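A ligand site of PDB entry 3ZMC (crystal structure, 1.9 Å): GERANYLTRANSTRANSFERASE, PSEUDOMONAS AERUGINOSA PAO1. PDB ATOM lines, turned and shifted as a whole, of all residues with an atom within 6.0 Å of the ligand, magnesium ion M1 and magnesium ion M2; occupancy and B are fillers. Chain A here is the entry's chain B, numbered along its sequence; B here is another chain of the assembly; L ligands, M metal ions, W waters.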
ATOM      1  N   ARG A  48       1.177  -9.391 -35.024  1.00  0.00           N
ATOM      2  CA  ARG A  48       1.194 -10.397 -36.062  1.00  0.00           C
ATOM      3  C   ARG A  48       0.048 -10.181 -37.062  1.00  0.00           C
ATOM      4  O   ARG A  48       0.238 -10.256 -38.249  1.00  0.00           O
ATOM      5  CB  ARG A  48       1.277 -11.797 -35.426  1.00  0.00           C
ATOM      6  CG  ARG A  48       2.688 -12.065 -34.846  1.00  0.00           C
ATOM      7  CD  ARG A  48       2.682 -13.082 -33.668  1.00  0.00           C
ATOM      8  NE  ARG A  48       4.024 -13.112 -33.051  1.00  0.00           N
ATOM      9  CZ  ARG A  48       4.443 -12.269 -32.130  1.00  0.00           C
ATOM     10  NH1 ARG A  48       3.636 -11.366 -31.568  1.00  0.00           N
ATOM     11  NH2 ARG A  48       5.690 -12.403 -31.663  1.00  0.00           N
ATOM     12  N   HIS A  77       0.126 -17.316 -31.588  1.00  0.00           N
ATOM     13  CA  HIS A  77       0.849 -16.495 -30.615  1.00  0.00           C
ATOM     14  C   HIS A  77       0.245 -16.648 -29.219  1.00  0.00           C
ATOM     15  O   HIS A  77       0.937 -16.896 -28.252  1.00  0.00           O
ATOM     16  CB  HIS A  77       0.838 -15.040 -31.055  1.00  0.00           C
ATOM     17  CG  HIS A  77       1.542 -14.114 -30.089  1.00  0.00           C
ATOM     18  ND1 HIS A  77       2.854 -14.304 -29.729  1.00  0.00           N
ATOM     19  CD2 HIS A  77       1.129 -13.006 -29.436  1.00  0.00           C
ATOM     20  CE1 HIS A  77       3.238 -13.308 -28.935  1.00  0.00           C
ATOM     21  NE2 HIS A  77       2.201 -12.522 -28.729  1.00  0.00           N
ATOM     22  N   TYR A  79      -1.581 -19.025 -27.900  1.00  0.00           N
ATOM     23  CA  TYR A  79      -1.471 -20.375 -27.268  1.00  0.00           C
ATOM     24  C   TYR A  79      -0.047 -20.478 -26.737  1.00  0.00           C
ATOM     25  O   TYR A  79       0.178 -20.944 -25.634  1.00  0.00           O
ATOM     26  CB  TYR A  79      -1.741 -21.530 -28.242  1.00  0.00           C
ATOM     27  CG  TYR A  79      -0.596 -22.395 -28.679  1.00  0.00           C
ATOM     28  CD1 TYR A  79      -0.024 -23.288 -27.797  1.00  0.00           C
ATOM     29  CD2 TYR A  79      -0.196 -22.465 -30.011  1.00  0.00           C
ATOM     30  CE1 TYR A  79       1.005 -24.119 -28.172  1.00  0.00           C
ATOM     31  CE2 TYR A  79       0.814 -23.314 -30.412  1.00  0.00           C
ATOM     32  CZ  TYR A  79       1.435 -24.122 -29.452  1.00  0.00           C
ATOM     33  OH  TYR A  79       2.497 -24.980 -29.780  1.00  0.00           O
ATOM     34  N   SER A  80       0.897 -19.990 -27.511  1.00  0.00           N
ATOM     35  CA  SER A  80       2.319 -20.034 -27.039  1.00  0.00           C
ATOM     36  C   SER A  80       2.563 -19.327 -25.709  1.00  0.00           C
ATOM     37  O   SER A  80       3.342 -19.770 -24.876  1.00  0.00           O
ATOM     38  CB  SER A  80       3.293 -19.485 -28.124  1.00  0.00           C
ATOM     39  OG  SER A  80       3.257 -18.031 -28.254  1.00  0.00           O
ATOM     40  N   LEU A  81       1.941 -18.190 -25.523  1.00  0.00           N
ATOM     41  CA  LEU A  81       2.124 -17.425 -24.303  1.00  0.00           C
ATOM     42  C   LEU A  81       1.472 -18.160 -23.115  1.00  0.00           C
ATOM     43  O   LEU A  81       2.021 -18.205 -22.030  1.00  0.00           O
ATOM     44  CB  LEU A  81       1.598 -16.006 -24.427  1.00  0.00           C
ATOM     45  CG  LEU A  81       2.139 -15.118 -25.513  1.00  0.00           C
ATOM     46  CD1 LEU A  81       1.675 -13.720 -25.252  1.00  0.00           C
ATOM     47  CD2 LEU A  81       3.667 -15.124 -25.459  1.00  0.00           C
ATOM     48  N   HIS A  83       1.213 -21.449 -22.721  1.00  0.00           N
ATOM     49  CA  HIS A  83       2.181 -22.512 -22.379  1.00  0.00           C
ATOM     50  C   HIS A  83       3.468 -22.015 -21.754  1.00  0.00           C
ATOM     51  O   HIS A  83       3.943 -22.605 -20.748  1.00  0.00           O
ATOM     52  CB  HIS A  83       2.451 -23.443 -23.569  1.00  0.00           C
ATOM     53  CG  HIS A  83       1.329 -24.432 -23.823  1.00  0.00           C
ATOM     54  ND1 HIS A  83       1.442 -25.487 -24.686  1.00  0.00           N
ATOM     55  CD2 HIS A  83       0.097 -24.556 -23.253  1.00  0.00           C
ATOM     56  CE1 HIS A  83       0.316 -26.171 -24.734  1.00  0.00           C
ATOM     57  NE2 HIS A  83      -0.521 -25.644 -23.861  1.00  0.00           N
ATOM     58  N   ASP A  84       3.997 -20.907 -22.282  1.00  0.00           N
ATOM     59  CA  ASP A  84       5.215 -20.296 -21.724  1.00  0.00           C
ATOM     60  C   ASP A  84       5.092 -19.921 -20.274  1.00  0.00           C
ATOM     61  O   ASP A  84       6.089 -20.005 -19.524  1.00  0.00           O
ATOM     62  CB  ASP A  84       5.558 -19.074 -22.589  1.00  0.00           C
ATOM     63  CG  ASP A  84       6.786 -18.307 -22.114  1.00  0.00           C
ATOM     64  OD1 ASP A  84       7.930 -18.793 -22.332  1.00  0.00           O
ATOM     65  OD2 ASP A  84       6.509 -17.228 -21.525  1.00  0.00           O
ATOM     66  N   ASP A  85       3.900 -19.477 -19.850  1.00  0.00           N
ATOM     67  CA  ASP A  85       3.641 -19.005 -18.543  1.00  0.00           C
ATOM     68  C   ASP A  85       3.553 -20.146 -17.538  1.00  0.00           C
ATOM     69  O   ASP A  85       3.628 -19.884 -16.342  1.00  0.00           O
ATOM     70  CB  ASP A  85       2.358 -18.144 -18.489  1.00  0.00           C
ATOM     71  CG  ASP A  85       2.534 -16.807 -19.096  1.00  0.00           C
ATOM     72  OD1 ASP A  85       3.654 -16.263 -19.066  1.00  0.00           O
ATOM     73  OD2 ASP A  85       1.533 -16.293 -19.621  1.00  0.00           O
ATOM     74  N   MET A  89       7.425 -24.076 -17.293  1.00  0.00           N
ATOM     75  CA  MET A  89       8.288 -23.208 -18.074  1.00  0.00           C
ATOM     76  C   MET A  89       8.613 -21.978 -17.251  1.00  0.00           C
ATOM     77  O   MET A  89       9.455 -22.062 -16.327  1.00  0.00           O
ATOM     78  CB  MET A  89       7.643 -22.924 -19.438  1.00  0.00           C
ATOM     79  CG  MET A  89       7.735 -24.210 -20.286  1.00  0.00           C
ATOM     80  SD  MET A  89       7.239 -24.221 -22.016  1.00  0.00           S
ATOM     81  CE  MET A  89       5.805 -25.243 -22.156  1.00  0.00           C
ATOM     82  N   ASP A  90       7.990 -20.854 -17.534  1.00  0.00           N
ATOM     83  CA  ASP A  90       8.415 -19.634 -16.857  1.00  0.00           C
ATOM     84  C   ASP A  90       7.713 -19.447 -15.529  1.00  0.00           C
ATOM     85  O   ASP A  90       8.145 -18.629 -14.722  1.00  0.00           O
ATOM     86  CB  ASP A  90       8.252 -18.436 -17.743  1.00  0.00           C
ATOM     87  CG  ASP A  90       9.181 -18.447 -18.874  1.00  0.00           C
ATOM     88  OD1 ASP A  90      10.221 -19.088 -18.742  1.00  0.00           O
ATOM     89  OD2 ASP A  90       8.971 -17.714 -19.871  1.00  0.00           O
ATOM     90  N   ASP A  92       4.880 -18.007 -14.529  1.00  0.00           N
ATOM     91  CA  ASP A  92       4.513 -16.658 -14.264  1.00  0.00           C
ATOM     92  C   ASP A  92       3.088 -16.488 -13.785  1.00  0.00           C
ATOM     93  O   ASP A  92       2.144 -17.034 -14.355  1.00  0.00           O
ATOM     94  CB  ASP A  92       4.789 -15.780 -15.491  1.00  0.00           C
ATOM     95  CG  ASP A  92       6.269 -15.374 -15.541  1.00  0.00           C
ATOM     96  OD1 ASP A  92       6.863 -15.063 -14.506  1.00  0.00           O
ATOM     97  OD2 ASP A  92       6.863 -15.409 -16.569  1.00  0.00           O
ATOM     98  N   ARG A  95       0.774 -11.663 -16.607  1.00  0.00           N
ATOM     99  CA  ARG A  95       1.232 -11.220 -17.887  1.00  0.00           C
ATOM    100  C   ARG A  95       0.631  -9.863 -18.086  1.00  0.00           C
ATOM    101  O   ARG A  95      -0.583  -9.665 -18.045  1.00  0.00           O
ATOM    102  CB  ARG A  95       0.826 -12.183 -18.970  1.00  0.00           C
ATOM    103  CG  ARG A  95       1.300 -11.757 -20.330  1.00  0.00           C
ATOM    104  CD  ARG A  95       1.190 -12.819 -21.417  1.00  0.00           C
ATOM    105  NE  ARG A  95       2.156 -13.859 -21.210  1.00  0.00           N
ATOM    106  CZ  ARG A  95       3.413 -13.839 -21.631  1.00  0.00           C
ATOM    107  NH1 ARG A  95       3.939 -12.761 -22.244  1.00  0.00           N
ATOM    108  NH2 ARG A  95       4.174 -14.897 -21.436  1.00  0.00           N
ATOM    109  N   ALA A 149       5.003 -22.851 -36.730  1.00  0.00           N
ATOM    110  CA  ALA A 149       4.516 -22.981 -35.354  1.00  0.00           C
ATOM    111  C   ALA A 149       5.049 -24.212 -34.667  1.00  0.00           C
ATOM    112  O   ALA A 149       5.031 -24.253 -33.439  1.00  0.00           O
ATOM    113  CB  ALA A 149       3.003 -23.051 -35.273  1.00  0.00           C
ATOM    114  N   MET A 154       8.668 -22.112 -33.983  1.00  0.00           N
ATOM    115  CA  MET A 154       8.378 -21.611 -32.695  1.00  0.00           C
ATOM    116  C   MET A 154       8.588 -22.580 -31.521  1.00  0.00           C
ATOM    117  O   MET A 154       9.154 -22.210 -30.505  1.00  0.00           O
ATOM    118  CB  MET A 154       6.931 -21.160 -32.655  1.00  0.00           C
ATOM    119  CG  MET A 154       6.486 -20.392 -31.455  1.00  0.00           C
ATOM    120  SD  MET A 154       4.702 -20.022 -31.453  1.00  0.00           S
ATOM    121  CE  MET A 154       3.955 -21.640 -31.173  1.00  0.00           C
ATOM    122  N   VAL A 155       8.007 -23.771 -31.611  1.00  0.00           N
ATOM    123  CA  VAL A 155       8.145 -24.779 -30.521  1.00  0.00           C
ATOM    124  C   VAL A 155       9.642 -25.102 -30.384  1.00  0.00           C
ATOM    125  O   VAL A 155      10.184 -25.273 -29.288  1.00  0.00           O
ATOM    126  CB  VAL A 155       7.321 -26.070 -30.773  1.00  0.00           C
ATOM    127  CG1 VAL A 155       7.658 -27.194 -29.752  1.00  0.00           C
ATOM    128  CG2 VAL A 155       5.885 -25.770 -30.624  1.00  0.00           C
ATOM    129  N   GLY A 157      12.188 -23.139 -31.049  1.00  0.00           N
ATOM    130  CA  GLY A 157      12.706 -22.034 -30.372  1.00  0.00           C
ATOM    131  C   GLY A 157      12.602 -22.063 -28.872  1.00  0.00           C
ATOM    132  O   GLY A 157      13.554 -21.743 -28.134  1.00  0.00           O
ATOM    133  N   GLN A 158      11.426 -22.434 -28.388  1.00  0.00           N
ATOM    134  CA  GLN A 158      11.196 -22.547 -26.992  1.00  0.00           C
ATOM    135  C   GLN A 158      12.044 -23.665 -26.385  1.00  0.00           C
ATOM    136  O   GLN A 158      12.616 -23.492 -25.316  1.00  0.00           O
ATOM    137  CB  GLN A 158       9.701 -22.812 -26.758  1.00  0.00           C
ATOM    138  CG  GLN A 158       9.343 -22.908 -25.270  1.00  0.00           C
ATOM    139  CD  GLN A 158       9.270 -21.512 -24.626  1.00  0.00           C
ATOM    140  OE1 GLN A 158       9.863 -20.556 -25.123  1.00  0.00           O
ATOM    141  NE2 GLN A 158       8.476 -21.377 -23.571  1.00  0.00           N
ATOM    142  N   ASP A 161      15.506 -22.278 -26.151  1.00  0.00           N
ATOM    143  CA  ASP A 161      15.450 -21.392 -25.012  1.00  0.00           C
ATOM    144  C   ASP A 161      15.596 -22.247 -23.691  1.00  0.00           C
ATOM    145  O   ASP A 161      16.500 -22.028 -22.874  1.00  0.00           O
ATOM    146  CB  ASP A 161      14.182 -20.506 -25.039  1.00  0.00           C
ATOM    147  CG  ASP A 161      14.177 -19.453 -23.974  1.00  0.00           C
ATOM    148  OD1 ASP A 161      15.019 -19.558 -23.085  1.00  0.00           O
ATOM    149  OD2 ASP A 161      13.368 -18.518 -23.969  1.00  0.00           O
ATOM    150  N   LEU A 162      14.771 -23.263 -23.523  1.00  0.00           N
ATOM    151  CA  LEU A 162      14.880 -24.060 -22.292  1.00  0.00           C
ATOM    152  C   LEU A 162      16.211 -24.894 -22.238  1.00  0.00           C
ATOM    153  O   LEU A 162      16.713 -25.163 -21.164  1.00  0.00           O
ATOM    154  CB  LEU A 162      13.608 -24.902 -22.077  1.00  0.00           C
ATOM    155  CG  LEU A 162      12.276 -24.123 -21.652  1.00  0.00           C
ATOM    156  CD1 LEU A 162      12.293 -23.380 -20.305  1.00  0.00           C
ATOM    157  CD2 LEU A 162      11.780 -23.114 -22.695  1.00  0.00           C
ATOM    158  N   LYS A 181      12.225 -18.917 -32.101  1.00  0.00           N
ATOM    159  CA  LYS A 181      11.250 -18.669 -31.085  1.00  0.00           C
ATOM    160  C   LYS A 181      10.270 -17.587 -31.491  1.00  0.00           C
ATOM    161  O   LYS A 181       9.055 -17.755 -31.313  1.00  0.00           O
ATOM    162  CB  LYS A 181      11.885 -18.327 -29.735  1.00  0.00           C
ATOM    163  CG  LYS A 181      10.910 -18.372 -28.583  1.00  0.00           C
ATOM    164  CD  LYS A 181      11.531 -18.114 -27.179  1.00  0.00           C
ATOM    165  CE  LYS A 181      11.647 -16.681 -26.786  1.00  0.00           C
ATOM    166  NZ  LYS A 181      12.231 -16.499 -25.426  1.00  0.00           N
ATOM    167  N   THR A 182      10.739 -16.494 -32.111  1.00  0.00           N
ATOM    168  CA  THR A 182       9.786 -15.478 -32.518  1.00  0.00           C
ATOM    169  C   THR A 182       9.856 -15.224 -34.063  1.00  0.00           C
ATOM    170  O   THR A 182       8.864 -14.787 -34.680  1.00  0.00           O
ATOM    171  CB  THR A 182       9.946 -14.160 -31.750  1.00  0.00           C
ATOM    172  OG1 THR A 182      11.347 -13.820 -31.732  1.00  0.00           O
ATOM    173  CG2 THR A 182       9.384 -14.208 -30.296  1.00  0.00           C
ATOM    174  N   LEU B 112       6.201 -29.459 -24.855  1.00  0.00           N
ATOM    175  CA  LEU B 112       6.637 -28.941 -26.155  1.00  0.00           C
ATOM    176  C   LEU B 112       6.617 -29.993 -27.253  1.00  0.00           C
ATOM    177  O   LEU B 112       6.126 -29.735 -28.342  1.00  0.00           O
ATOM    178  CB  LEU B 112       8.071 -28.343 -26.077  1.00  0.00           C
ATOM    179  CG  LEU B 112       8.180 -27.113 -25.229  1.00  0.00           C
ATOM    180  CD1 LEU B 112       9.649 -26.697 -25.093  1.00  0.00           C
ATOM    181  CD2 LEU B 112       7.369 -25.971 -25.826  1.00  0.00           C
ATOM    182  N   ASP B 115       3.210 -30.388 -28.308  1.00  0.00           N
ATOM    183  CA  ASP B 115       2.747 -29.233 -29.094  1.00  0.00           C
ATOM    184  C   ASP B 115       3.244 -29.342 -30.572  1.00  0.00           C
ATOM    185  O   ASP B 115       2.536 -28.945 -31.519  1.00  0.00           O
ATOM    186  CB  ASP B 115       3.237 -27.922 -28.541  1.00  0.00           C
ATOM    187  CG  ASP B 115       2.522 -27.527 -27.209  1.00  0.00           C
ATOM    188  OD1 ASP B 115       1.396 -27.972 -26.985  1.00  0.00           O
ATOM    189  OD2 ASP B 115       3.122 -26.708 -26.393  1.00  0.00           O
HETATM  190  C1  LIG L   1       7.668 -16.200 -24.871  1.00  0.00           C
HETATM  191  O1  LIG L   1       9.051 -15.815 -24.560  1.00  0.00           O
HETATM  192  C2  LIG L   1       7.569 -17.413 -25.763  1.00  0.00           C
HETATM  193  C3  LIG L   1       7.076 -17.345 -27.032  1.00  0.00           C
HETATM  194  C4  LIG L   1       6.702 -16.072 -27.683  1.00  0.00           C
HETATM  195  C5  LIG L   1       6.919 -18.485 -27.991  1.00  0.00           C
HETATM  196  C6  LIG L   1       7.422 -19.876 -27.645  1.00  0.00           C
HETATM  197  C7  LIG L   1       6.570 -20.582 -26.669  1.00  0.00           C
HETATM  198  C8  LIG L   1       6.019 -21.831 -26.811  1.00  0.00           C
HETATM  199  C9  LIG L   1       6.139 -22.676 -28.022  1.00  0.00           C
HETATM  200  C10 LIG L   1       5.257 -22.397 -25.650  1.00  0.00           C
HETATM  201  P1  LIG L   1       9.529 -15.302 -23.175  1.00  0.00           P
HETATM  202  O2  LIG L   1       9.143 -16.244 -22.055  1.00  0.00           O
HETATM  203  O3  LIG L   1      10.991 -14.981 -23.385  1.00  0.00           O
HETATM  204  O4  LIG L   1       8.736 -13.954 -23.167  1.00  0.00           O
HETATM  205  P2  LIG L   1       7.727 -13.312 -22.092  1.00  0.00           P
HETATM  206  O5  LIG L   1       7.263 -14.478 -21.243  1.00  0.00           O
HETATM  207  O6  LIG L   1       8.609 -12.374 -21.439  1.00  0.00           O
HETATM  208  O7  LIG L   1       6.680 -12.647 -22.929  1.00  0.00           O
HETATM  209 MG    MG M   1       7.932 -16.055 -20.362  1.00  0.00          MG
HETATM  210 MG    MG M   2       9.768 -18.144 -21.724  1.00  0.00          MG
HETATM  211  O   HOH W   1      11.732 -17.359 -21.077  1.00  0.00           O
HETATM  212  O   HOH W   2      10.300 -20.105 -21.190  1.00  0.00           O
HETATM  213  O   HOH W   3       6.595 -10.027 -22.199  1.00  0.00           O
HETATM  214  O   HOH W   4       9.162 -14.882 -19.157  1.00  0.00           O
HETATM  215  O   HOH W   5      10.448 -18.517 -23.480  1.00  0.00           O
HETATM  216  O   HOH W   6       6.117 -12.841 -19.108  1.00  0.00           O
HETATM  217  O   HOH W   7       6.286 -12.507 -25.813  1.00  0.00           O
HETATM  218  O   HOH W   8       6.472 -15.996 -18.859  1.00  0.00           O
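Residues that only touch the ligand: Ser 80 (3.3 Å), Gln 158 (3.5 Å), His 83 (3.6 Å), Val 155 (3.8 Å), Leu 81 (3.9 Å) and Met 154 (3.9 Å). Within 4 Å of the ligand: Ser 80, Leu 81, His 83, Asp 84, Asp 90, Arg 95, Met 154, Val 155, Gln 158 and Lys 181. The nearest printed residue that does not touch the ligand is Leu 112 of chain B (4.1 Å).
An oxygen (O7) of the ligand lies within salt-bridge range of the guanidinium group of Arg 95 (2.8 Å). The side-chain amino group (NZ) of Lys 181 lies within salt-bridge range of an oxygen (O3) of the ligand (2.8 Å).
The side-chain carboxylate of Asp 84 lies close to the guanidinium group of Arg 95 (3.3 Å). NE2 of Gln 158 lies close to OD1 of Asp 84 (2.9 Å). The guanidinium group of Arg 95 is in salt-bridge range of the side-chain carboxylate of Asp 85 (2.8 Å). The side-chain carboxylate (OD2) of Asp 161 is in salt-bridge range of the side-chain amino group (NZ) of Lys 181. OG of Ser 80 lies within hydrogen-bond range of O of His 77 (2.6 Å). The side-chain amide nitrogen (NE2) of Gln 158 sits at hydrogen-bond distance from the side-chain sulfur (SD) of Met 89 (3.5 Å). The side-chain carboxylate (OD2) of Asp 115 of chain B is in hydrogen-bond range of a ring nitrogen (ND1) of His 83, 2.7 Å away. The backbone NH of Asp 92 is in hydrogen-bond range of the backbone carbonyl oxygen of Asp 85.
Residues that only touch magnesium ion M2: Gln 158 (3.9 Å). Of the 23 residues printed, 3 come within 4 Å of magnesium ion M2.
Magnesium ion M1 is bound by O5 of the ligand (1.9 Å), OD2 of Asp 90 (2.0 Å), water W4 (2.1 Å), O2 of the ligand (2.1 Å), water W8 (2.1 Å) and OD2 of Asp 84 (2.2 Å). Magnesium ion M1 has six donor atoms within binding distance.
Magnesium ion M2 is bound by water W5 (1.9 Å), O2 of the ligand (2.0 Å), OD1 of Asp 84 (2.0 Å), OD2 of Asp 90 (2.1 Å), water W2 (2.1 Å) and water W1 (2.2 Å). Magnesium ion M2 has six donor atoms within binding distance.
Water W2 lies within hydrogen-bond range of OD1 of Asp 90 (2.7 Å) and NE2 of Gln 158 (3.3 Å). Water W1 lies within hydrogen-bond range of the side-chain carboxylate (OD1) of Asp 90 (3.3 Å) and an oxygen (O3) of the ligand (3.4 Å).
Asp 92 touches magnesium ion M1 (OD2 to MG, 3.99 Å). Three residues have an atom within 4 Å of magnesium ion M1: Asp 84, Asp 90 and Asp 92. The nearest printed residue that does not touch magnesium ion M1 is Arg 95 (4.1 Å).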
